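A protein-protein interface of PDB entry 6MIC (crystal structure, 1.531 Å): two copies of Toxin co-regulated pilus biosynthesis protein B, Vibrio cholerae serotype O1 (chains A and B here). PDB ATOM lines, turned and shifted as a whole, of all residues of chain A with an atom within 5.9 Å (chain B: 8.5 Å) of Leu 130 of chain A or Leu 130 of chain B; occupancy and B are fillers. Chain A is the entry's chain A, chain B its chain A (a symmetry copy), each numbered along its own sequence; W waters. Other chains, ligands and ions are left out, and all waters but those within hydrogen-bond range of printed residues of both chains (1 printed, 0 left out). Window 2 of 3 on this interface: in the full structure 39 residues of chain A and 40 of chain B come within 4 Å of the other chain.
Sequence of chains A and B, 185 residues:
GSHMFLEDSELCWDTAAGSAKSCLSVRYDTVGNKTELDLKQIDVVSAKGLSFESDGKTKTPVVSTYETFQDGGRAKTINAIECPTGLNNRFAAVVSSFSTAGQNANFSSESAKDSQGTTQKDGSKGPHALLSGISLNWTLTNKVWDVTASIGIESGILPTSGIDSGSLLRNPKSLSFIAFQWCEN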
ATOM      1  N   THR A 100       6.814  -5.083 -19.717  1.00  0.00           N
ATOM      2  CA  THR A 100       7.034  -5.675 -18.402  1.00  0.00           C
ATOM      3  C   THR A 100       6.179  -5.037 -17.309  1.00  0.00           C
ATOM      4  O   THR A 100       6.497  -5.183 -16.117  1.00  0.00           O
ATOM      5  CB  THR A 100       8.510  -5.565 -18.059  1.00  0.00           C
ATOM      6  OG1 THR A 100       8.872  -4.188 -18.168  1.00  0.00           O
ATOM      7  CG2 THR A 100       9.327  -6.390 -19.041  1.00  0.00           C
ATOM      8  N   HIS A 128       9.705   0.410 -15.895  1.00  0.00           N
ATOM      9  CA  HIS A 128       9.597  -0.886 -16.537  1.00  0.00           C
ATOM     10  C   HIS A 128      10.894  -1.669 -16.375  1.00  0.00           C
ATOM     11  O   HIS A 128      11.987  -1.161 -16.644  1.00  0.00           O
ATOM     12  CB  HIS A 128       9.239  -0.720 -18.015  1.00  0.00           C
ATOM     13  CG  HIS A 128       7.834  -0.255 -18.257  1.00  0.00           C
ATOM     14  ND1 HIS A 128       7.466   1.076 -18.250  1.00  0.00           N
ATOM     15  CD2 HIS A 128       6.702  -0.951 -18.514  1.00  0.00           C
ATOM     16  CE1 HIS A 128       6.173   1.174 -18.511  1.00  0.00           C
ATOM     17  NE2 HIS A 128       5.682  -0.042 -18.654  1.00  0.00           N
ATOM     18  N   ALA A 129      10.762  -2.907 -15.898  1.00  0.00           N
ATOM     19  CA  ALA A 129      11.858  -3.834 -15.804  1.00  0.00           C
ATOM     20  C   ALA A 129      12.265  -4.335 -17.180  1.00  0.00           C
ATOM     21  O   ALA A 129      11.541  -4.185 -18.173  1.00  0.00           O
ATOM     22  CB  ALA A 129      11.457  -5.002 -14.906  1.00  0.00           C
ATOM     23  N   LEU A 130      13.451  -4.913 -17.231  1.00  0.00           N
ATOM     24  CA  LEU A 130      13.975  -5.540 -18.435  1.00  0.00           C
ATOM     25  C   LEU A 130      13.494  -6.978 -18.529  1.00  0.00           C
ATOM     26  O   LEU A 130      13.179  -7.622 -17.535  1.00  0.00           O
ATOM     27  CB  LEU A 130      15.498  -5.454 -18.450  1.00  0.00           C
ATOM     28  CG  LEU A 130      15.971  -3.991 -18.419  1.00  0.00           C
ATOM     29  CD1 LEU A 130      17.484  -3.937 -18.286  1.00  0.00           C
ATOM     30  CD2 LEU A 130      15.537  -3.194 -19.640  1.00  0.00           C
ATOM     31  N   LEU A 131      13.435  -7.473 -19.757  1.00  0.00           N
ATOM     32  CA  LEU A 131      12.731  -8.707 -20.093  1.00  0.00           C
ATOM     33  C   LEU A 131      13.683  -9.847 -20.466  1.00  0.00           C
ATOM     34  O   LEU A 131      14.697  -9.631 -21.129  1.00  0.00           O
ATOM     35  CB  LEU A 131      11.751  -8.387 -21.240  1.00  0.00           C
ATOM     36  CG  LEU A 131      10.801  -9.482 -21.718  1.00  0.00           C
ATOM     37  CD1 LEU A 131       9.457  -8.906 -22.115  1.00  0.00           C
ATOM     38  CD2 LEU A 131      11.468 -10.152 -22.884  1.00  0.00           C
ATOM     39  N   SER A 132      13.349 -11.071 -20.042  1.00  0.00           N
ATOM     40  CA  SER A 132      14.044 -12.287 -20.452  1.00  0.00           C
ATOM     41  C   SER A 132      13.219 -13.256 -21.306  1.00  0.00           C
ATOM     42  O   SER A 132      13.812 -14.157 -21.917  1.00  0.00           O
ATOM     43  CB  SER A 132      14.547 -13.059 -19.228  1.00  0.00           C
ATOM     44  OG  SER A 132      13.496 -13.422 -18.354  1.00  0.00           O
ATOM     45  N   GLY A 152       8.943 -13.193 -18.327  1.00  0.00           N
ATOM     46  CA  GLY A 152      10.064 -13.260 -17.418  1.00  0.00           C
ATOM     47  C   GLY A 152      10.816 -11.946 -17.475  1.00  0.00           C
ATOM     48  O   GLY A 152      10.993 -11.343 -18.545  1.00  0.00           O
ATOM     49  N   ILE A 153      11.210 -11.490 -16.285  1.00  0.00           N
ATOM     50  CA  ILE A 153      11.868 -10.209 -16.101  1.00  0.00           C
ATOM     51  C   ILE A 153      13.081 -10.362 -15.192  1.00  0.00           C
ATOM     52  O   ILE A 153      13.293 -11.390 -14.549  1.00  0.00           O
ATOM     53  CB  ILE A 153      10.917  -9.129 -15.548  1.00  0.00           C
ATOM     54  CG1 ILE A 153      10.477  -9.368 -14.104  1.00  0.00           C
ATOM     55  CG2 ILE A 153       9.706  -9.004 -16.458  1.00  0.00           C
ATOM     56  CD1 ILE A 153       9.983  -8.090 -13.454  1.00  0.00           C
ATOM     57  N   GLU A 154      13.897  -9.307 -15.175  1.00  0.00           N
ATOM     58  CA  GLU A 154      15.052  -9.268 -14.292  1.00  0.00           C
ATOM     59  C   GLU A 154      14.613  -9.500 -12.850  1.00  0.00           C
ATOM     60  O   GLU A 154      13.546  -9.052 -12.404  1.00  0.00           O
ATOM     61  CB  GLU A 154      15.793  -7.937 -14.424  1.00  0.00           C
ATOM     62  CG  GLU A 154      15.050  -6.740 -13.939  1.00  0.00           C
ATOM     63  CD  GLU A 154      15.794  -5.437 -14.214  1.00  0.00           C
ATOM     64  OE1 GLU A 154      16.935  -5.275 -13.730  1.00  0.00           O
ATOM     65  OE2 GLU A 154      15.234  -4.566 -14.901  1.00  0.00           O
ATOM     66  N   ILE A 157      13.210  -7.260  -8.397  1.00  0.00           N
ATOM     67  CA  ILE A 157      12.343  -6.101  -8.544  1.00  0.00           C
ATOM     68  C   ILE A 157      10.984  -6.350  -7.906  1.00  0.00           C
ATOM     69  O   ILE A 157      10.508  -5.550  -7.090  1.00  0.00           O
ATOM     70  CB  ILE A 157      12.200  -5.704 -10.026  1.00  0.00           C
ATOM     71  CG1 ILE A 157      13.548  -5.170 -10.507  1.00  0.00           C
ATOM     72  CG2 ILE A 157      11.099  -4.650 -10.206  1.00  0.00           C
ATOM     73  CD1 ILE A 157      13.577  -4.756 -11.908  1.00  0.00           C
ATOM     74  N   SER B  99      12.556 -17.259 -25.057  1.00  0.00           N
ATOM     75  CA  SER B  99      13.314 -16.917 -23.860  1.00  0.00           C
ATOM     76  C   SER B  99      14.776 -16.855 -24.253  1.00  0.00           C
ATOM     77  O   SER B  99      15.150 -17.159 -25.388  1.00  0.00           O
ATOM     78  CB  SER B  99      13.098 -17.911 -22.722  1.00  0.00           C
ATOM     79  OG  SER B  99      13.889 -19.067 -22.912  1.00  0.00           O
ATOM     80  N   THR B 100      15.618 -16.473 -23.295  1.00  0.00           N
ATOM     81  CA  THR B 100      17.063 -16.419 -23.489  1.00  0.00           C
ATOM     82  C   THR B 100      17.770 -17.708 -23.073  1.00  0.00           C
ATOM     83  O   THR B 100      18.992 -17.693 -22.851  1.00  0.00           O
ATOM     84  CB  THR B 100      17.615 -15.233 -22.716  1.00  0.00           C
ATOM     85  OG1 THR B 100      17.193 -15.374 -21.359  1.00  0.00           O
ATOM     86  CG2 THR B 100      17.058 -13.941 -23.293  1.00  0.00           C
ATOM     87  N   ALA B 101      17.050 -18.833 -23.015  1.00  0.00           N
ATOM     88  CA  ALA B 101      17.700 -20.073 -22.623  1.00  0.00           C
ATOM     89  C   ALA B 101      18.538 -20.680 -23.741  1.00  0.00           C
ATOM     90  O   ALA B 101      19.417 -21.504 -23.455  1.00  0.00           O
ATOM     91  CB  ALA B 101      16.666 -21.074 -22.133  1.00  0.00           C
ATOM     92  N   THR B 118      20.233 -19.684 -19.127  1.00  0.00           N
ATOM     93  CA  THR B 118      21.262 -19.337 -20.108  1.00  0.00           C
ATOM     94  C   THR B 118      22.580 -19.995 -19.731  1.00  0.00           C
ATOM     95  O   THR B 118      22.969 -20.001 -18.558  1.00  0.00           O
ATOM     96  CB  THR B 118      21.447 -17.816 -20.185  1.00  0.00           C
ATOM     97  OG1 THR B 118      20.183 -17.167 -20.417  1.00  0.00           O
ATOM     98  CG2 THR B 118      22.409 -17.433 -21.288  1.00  0.00           C
ATOM     99  N   PRO B 127      20.913 -18.291 -14.513  1.00  0.00           N
ATOM    100  CA  PRO B 127      19.630 -17.617 -14.696  1.00  0.00           C
ATOM    101  C   PRO B 127      19.453 -17.208 -16.143  1.00  0.00           C
ATOM    102  O   PRO B 127      20.400 -17.193 -16.930  1.00  0.00           O
ATOM    103  CB  PRO B 127      19.718 -16.402 -13.772  1.00  0.00           C
ATOM    104  CG  PRO B 127      21.159 -16.196 -13.542  1.00  0.00           C
ATOM    105  CD  PRO B 127      21.830 -17.531 -13.654  1.00  0.00           C
ATOM    106  N   HIS B 128      18.213 -16.898 -16.497  1.00  0.00           N
ATOM    107  CA  HIS B 128      17.946 -16.355 -17.815  1.00  0.00           C
ATOM    108  C   HIS B 128      18.544 -14.959 -17.945  1.00  0.00           C
ATOM    109  O   HIS B 128      18.340 -14.093 -17.089  1.00  0.00           O
ATOM    110  CB  HIS B 128      16.441 -16.335 -18.089  1.00  0.00           C
ATOM    111  CG  HIS B 128      15.839 -17.692 -18.300  1.00  0.00           C
ATOM    112  ND1 HIS B 128      15.412 -18.500 -17.266  1.00  0.00           N
ATOM    113  CD2 HIS B 128      15.591 -18.382 -19.438  1.00  0.00           C
ATOM    114  CE1 HIS B 128      14.913 -19.619 -17.763  1.00  0.00           C
ATOM    115  NE2 HIS B 128      15.029 -19.582 -19.076  1.00  0.00           N
ATOM    116  N   ALA B 129      19.313 -14.762 -19.014  1.00  0.00           N
ATOM    117  CA  ALA B 129      19.851 -13.474 -19.370  1.00  0.00           C
ATOM    118  C   ALA B 129      18.761 -12.559 -19.902  1.00  0.00           C
ATOM    119  O   ALA B 129      17.655 -12.990 -20.251  1.00  0.00           O
ATOM    120  CB  ALA B 129      20.953 -13.656 -20.411  1.00  0.00           C
ATOM    121  N   LEU B 130      19.080 -11.279 -19.934  1.00  0.00           N
ATOM    122  CA  LEU B 130      18.207 -10.259 -20.498  1.00  0.00           C
ATOM    123  C   LEU B 130      18.434 -10.147 -21.996  1.00  0.00           C
ATOM    124  O   LEU B 130      19.496 -10.465 -22.517  1.00  0.00           O
ATOM    125  CB  LEU B 130      18.436  -8.926 -19.793  1.00  0.00           C
ATOM    126  CG  LEU B 130      18.142  -9.038 -18.287  1.00  0.00           C
ATOM    127  CD1 LEU B 130      18.518  -7.742 -17.588  1.00  0.00           C
ATOM    128  CD2 LEU B 130      16.692  -9.381 -17.982  1.00  0.00           C
ATOM    129  N   LEU B 131      17.400  -9.690 -22.688  1.00  0.00           N
ATOM    130  CA  LEU B 131      17.301  -9.784 -24.142  1.00  0.00           C
ATOM    131  C   LEU B 131      17.430  -8.423 -24.832  1.00  0.00           C
ATOM    132  O   LEU B 131      16.922  -7.416 -24.341  1.00  0.00           O
ATOM    133  CB  LEU B 131      15.957 -10.463 -24.476  1.00  0.00           C
ATOM    134  CG  LEU B 131      15.642 -10.789 -25.932  1.00  0.00           C
ATOM    135  CD1 LEU B 131      14.874 -12.089 -26.050  1.00  0.00           C
ATOM    136  CD2 LEU B 131      14.844  -9.638 -26.469  1.00  0.00           C
ATOM    137  N   SER B 132      18.112  -8.395 -25.983  1.00  0.00           N
ATOM    138  CA  SER B 132      18.183  -7.228 -26.854  1.00  0.00           C
ATOM    139  C   SER B 132      17.501  -7.385 -28.217  1.00  0.00           C
ATOM    140  O   SER B 132      17.277  -6.366 -28.888  1.00  0.00           O
ATOM    141  CB  SER B 132      19.641  -6.831 -27.108  1.00  0.00           C
ATOM    142  OG  SER B 132      20.383  -7.877 -27.705  1.00  0.00           O
ATOM    143  N   GLY B 133      17.178  -8.585 -28.661  1.00  0.00           N
ATOM    144  CA  GLY B 133      16.477  -8.701 -29.931  1.00  0.00           C
ATOM    145  C   GLY B 133      16.268 -10.143 -30.338  1.00  0.00           C
ATOM    146  O   GLY B 133      16.867 -11.074 -29.784  1.00  0.00           O
ATOM    147  N   ILE B 151      18.829 -14.868 -31.168  1.00  0.00           N
ATOM    148  CA  ILE B 151      18.382 -14.045 -30.049  1.00  0.00           C
ATOM    149  C   ILE B 151      19.609 -13.357 -29.473  1.00  0.00           C
ATOM    150  O   ILE B 151      20.601 -14.017 -29.161  1.00  0.00           O
ATOM    151  CB  ILE B 151      17.658 -14.896 -28.991  1.00  0.00           C
ATOM    152  CG1 ILE B 151      16.407 -15.521 -29.603  1.00  0.00           C
ATOM    153  CG2 ILE B 151      17.349 -14.053 -27.746  1.00  0.00           C
ATOM    154  CD1 ILE B 151      15.653 -16.449 -28.678  1.00  0.00           C
ATOM    155  N   GLY B 152      19.551 -12.033 -29.384  1.00  0.00           N
ATOM    156  CA  GLY B 152      20.623 -11.254 -28.810  1.00  0.00           C
ATOM    157  C   GLY B 152      20.337 -11.039 -27.339  1.00  0.00           C
ATOM    158  O   GLY B 152      19.190 -10.807 -26.926  1.00  0.00           O
ATOM    159  N   ILE B 153      21.404 -11.172 -26.550  1.00  0.00           N
ATOM    160  CA  ILE B 153      21.338 -11.095 -25.101  1.00  0.00           C
ATOM    161  C   ILE B 153      22.451 -10.202 -24.567  1.00  0.00           C
ATOM    162  O   ILE B 153      23.381  -9.817 -25.276  1.00  0.00           O
ATOM    163  CB  ILE B 153      21.396 -12.482 -24.430  1.00  0.00           C
ATOM    164  CG1 ILE B 153      22.749 -13.180 -24.560  1.00  0.00           C
ATOM    165  CG2 ILE B 153      20.289 -13.362 -24.989  1.00  0.00           C
ATOM    166  CD1 ILE B 153      22.923 -14.256 -23.505  1.00  0.00           C
ATOM    167  N   GLU B 154      22.318  -9.857 -23.286  1.00  0.00           N
ATOM    168  CA  GLU B 154      23.343  -9.078 -22.609  1.00  0.00           C
ATOM    169  C   GLU B 154      24.693  -9.778 -22.731  1.00  0.00           C
ATOM    170  O   GLU B 154      24.804 -11.013 -22.692  1.00  0.00           O
ATOM    171  CB  GLU B 154      22.979  -8.860 -21.140  1.00  0.00           C
ATOM    172  CG  GLU B 154      22.976 -10.084 -20.292  1.00  0.00           C
ATOM    173  CD  GLU B 154      22.485  -9.814 -18.873  1.00  0.00           C
ATOM    174  OE1 GLU B 154      23.097  -8.984 -18.166  1.00  0.00           O
ATOM    175  OE2 GLU B 154      21.496 -10.441 -18.456  1.00  0.00           O
ATOM    176  N   SER B 155      25.732  -8.964 -22.882  1.00  0.00           N
ATOM    177  CA  SER B 155      27.071  -9.495 -23.048  1.00  0.00           C
ATOM    178  C   SER B 155      27.655  -9.908 -21.703  1.00  0.00           C
ATOM    179  O   SER B 155      27.147  -9.571 -20.634  1.00  0.00           O
ATOM    180  CB  SER B 155      28.000  -8.474 -23.701  1.00  0.00           C
ATOM    181  OG  SER B 155      28.136  -7.329 -22.882  1.00  0.00           O
ATOM    182  N   ILE B 157      28.035 -13.041 -20.494  1.00  0.00           N
ATOM    183  CA  ILE B 157      27.424 -14.191 -19.849  1.00  0.00           C
ATOM    184  C   ILE B 157      27.857 -15.489 -20.516  1.00  0.00           C
ATOM    185  O   ILE B 157      28.324 -16.422 -19.850  1.00  0.00           O
ATOM    186  CB  ILE B 157      25.888 -14.061 -19.827  1.00  0.00           C
ATOM    187  CG1 ILE B 157      25.521 -12.918 -18.882  1.00  0.00           C
ATOM    188  CG2 ILE B 157      25.233 -15.374 -19.378  1.00  0.00           C
ATOM    189  CD1 ILE B 157      24.088 -12.662 -18.759  1.00  0.00           C
ATOM    190  N   SER B 167      27.277 -12.836 -27.531  1.00  0.00           N
ATOM    191  CA  SER B 167      26.007 -12.266 -27.117  1.00  0.00           C
ATOM    192  C   SER B 167      24.850 -12.836 -27.926  1.00  0.00           C
ATOM    193  O   SER B 167      23.781 -12.226 -27.980  1.00  0.00           O
ATOM    194  CB  SER B 167      26.030 -10.742 -27.254  1.00  0.00           C
ATOM    195  OG  SER B 167      27.051 -10.189 -26.436  1.00  0.00           O
ATOM    196  N   LEU B 169      22.380 -16.251 -29.252  1.00  0.00           N
ATOM    197  CA  LEU B 169      21.847 -17.605 -29.191  1.00  0.00           C
ATOM    198  C   LEU B 169      21.421 -17.979 -30.601  1.00  0.00           C
ATOM    199  O   LEU B 169      20.474 -17.397 -31.144  1.00  0.00           O
ATOM    200  CB  LEU B 169      20.667 -17.679 -28.232  1.00  0.00           C
ATOM    201  CG  LEU B 169      20.817 -16.963 -26.900  1.00  0.00           C
ATOM    202  CD1 LEU B 169      19.496 -16.999 -26.152  1.00  0.00           C
ATOM    203  CD2 LEU B 169      21.947 -17.586 -26.068  1.00  0.00           C
HETATM  204  O   HOH W   1      15.971  -7.065 -21.613  1.00  0.00           O
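O of Leu 131 of chain A is in hydrogen-bond range of N of Leu 131 of chain B (3.1 Å).
The backbone NH (N) of Thr 100 of chain B sits at hydrogen-bond distance from the backbone carbonyl oxygen (O) of Ser 132 of chain A (3.2 Å).
N of Leu 130 of chain A lies within hydrogen-bond range of OE2 of Glu 154 of chain A (3.0 Å).
The backbone NH (N) of Ser 132 of chain A sits at hydrogen-bond distance from the backbone carbonyl oxygen (O) of Gly 152 of chain A (2.8 Å).
The side-chain hydroxyl of Thr 118 of chain B is in hydrogen-bond range of the backbone carbonyl oxygen of Thr 100 of chain B, 2.8 Å away.
The backbone carbonyl oxygen (O) of Ala 129 of chain B lies within hydrogen-bond range of the side-chain hydroxyl (OG1) of Thr 100 of chain B, 2.7 Å away.
The side-chain hydroxyl of Thr 118 of chain B lies within hydrogen-bond range of the backbone NH of Ala 129 of chain B.
The backbone NH of Leu 130 of chain B lies within hydrogen-bond range of the side-chain carboxylate of Glu 154 of chain B, 3.0 Å away.
Among the printed residues, merely in contact across the chains: Ser 132 of chain A with Ala 129 of chain B, Ser 132 of chain A with Ser 99 of chain B, Leu 131 of chain A with Leu 130 of chain B, Leu 130 of chain A with Leu 130 of chain B, Glu 154 of chain A with Leu 130 of chain B and Ser 132 of chain A with His 128 of chain B.
Of chain B, only Leu 130 (3.9 Å) comes within 4 Å of Leu 130 of chain A.
No residue of chain B comes within 4 Å of Ala 129 of chain A.
Of the printed residues of chain B, Glu 154 of chain A touches Leu 130.
Of the printed residues of chain B, Leu 131 of chain A touches Leu 130 (3.6 Å) and Leu 131 (3.1 Å).
Gly 152 of chain A touches none of the printed residues of chain B.
The nearest residue of chain A that does not touch Leu 130 of chain B is Ser 132 of chain A (4.3 Å).
Of the 19 printed residues of chain B, 6 touch a printed residue of chain A.
Of the 10 printed residues of chain A, 4 touch a printed residue of chain B.
Among the printed residues, no Asp or Glu carboxylate lies within 4 Å of a Lys or Arg side-chain nitrogen of the other chain.
Leu 131 of chain A touches its own counterpart, Leu 131 of chain B.
Ser 132 of chain A touches His 128 of chain B, but with the chains exchanged His 128 of chain A does not touch Ser 132 of chain B (13.3 Å).
Ser 132 of chain A touches Ala 129 of chain B, but with the chains exchanged Ala 129 of chain A does not touch Ser 132 of chain B (11.0 Å).
Glu 154 of chain A touches Leu 130 of chain B, but with the chains exchanged Leu 130 of chain A does not touch Glu 154 of chain B (7.5 Å).
Of the 8 pairs that touch across the chains among the printed residues, 2 have their exchanged pair printed and touching as well.
Water W1 bridges the backbone carbonyl oxygen (O) of Leu 131 of chain A (2.9 Å) and the backbone carbonyl oxygen (O) of Leu 131 of chain B (2.9 Å).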
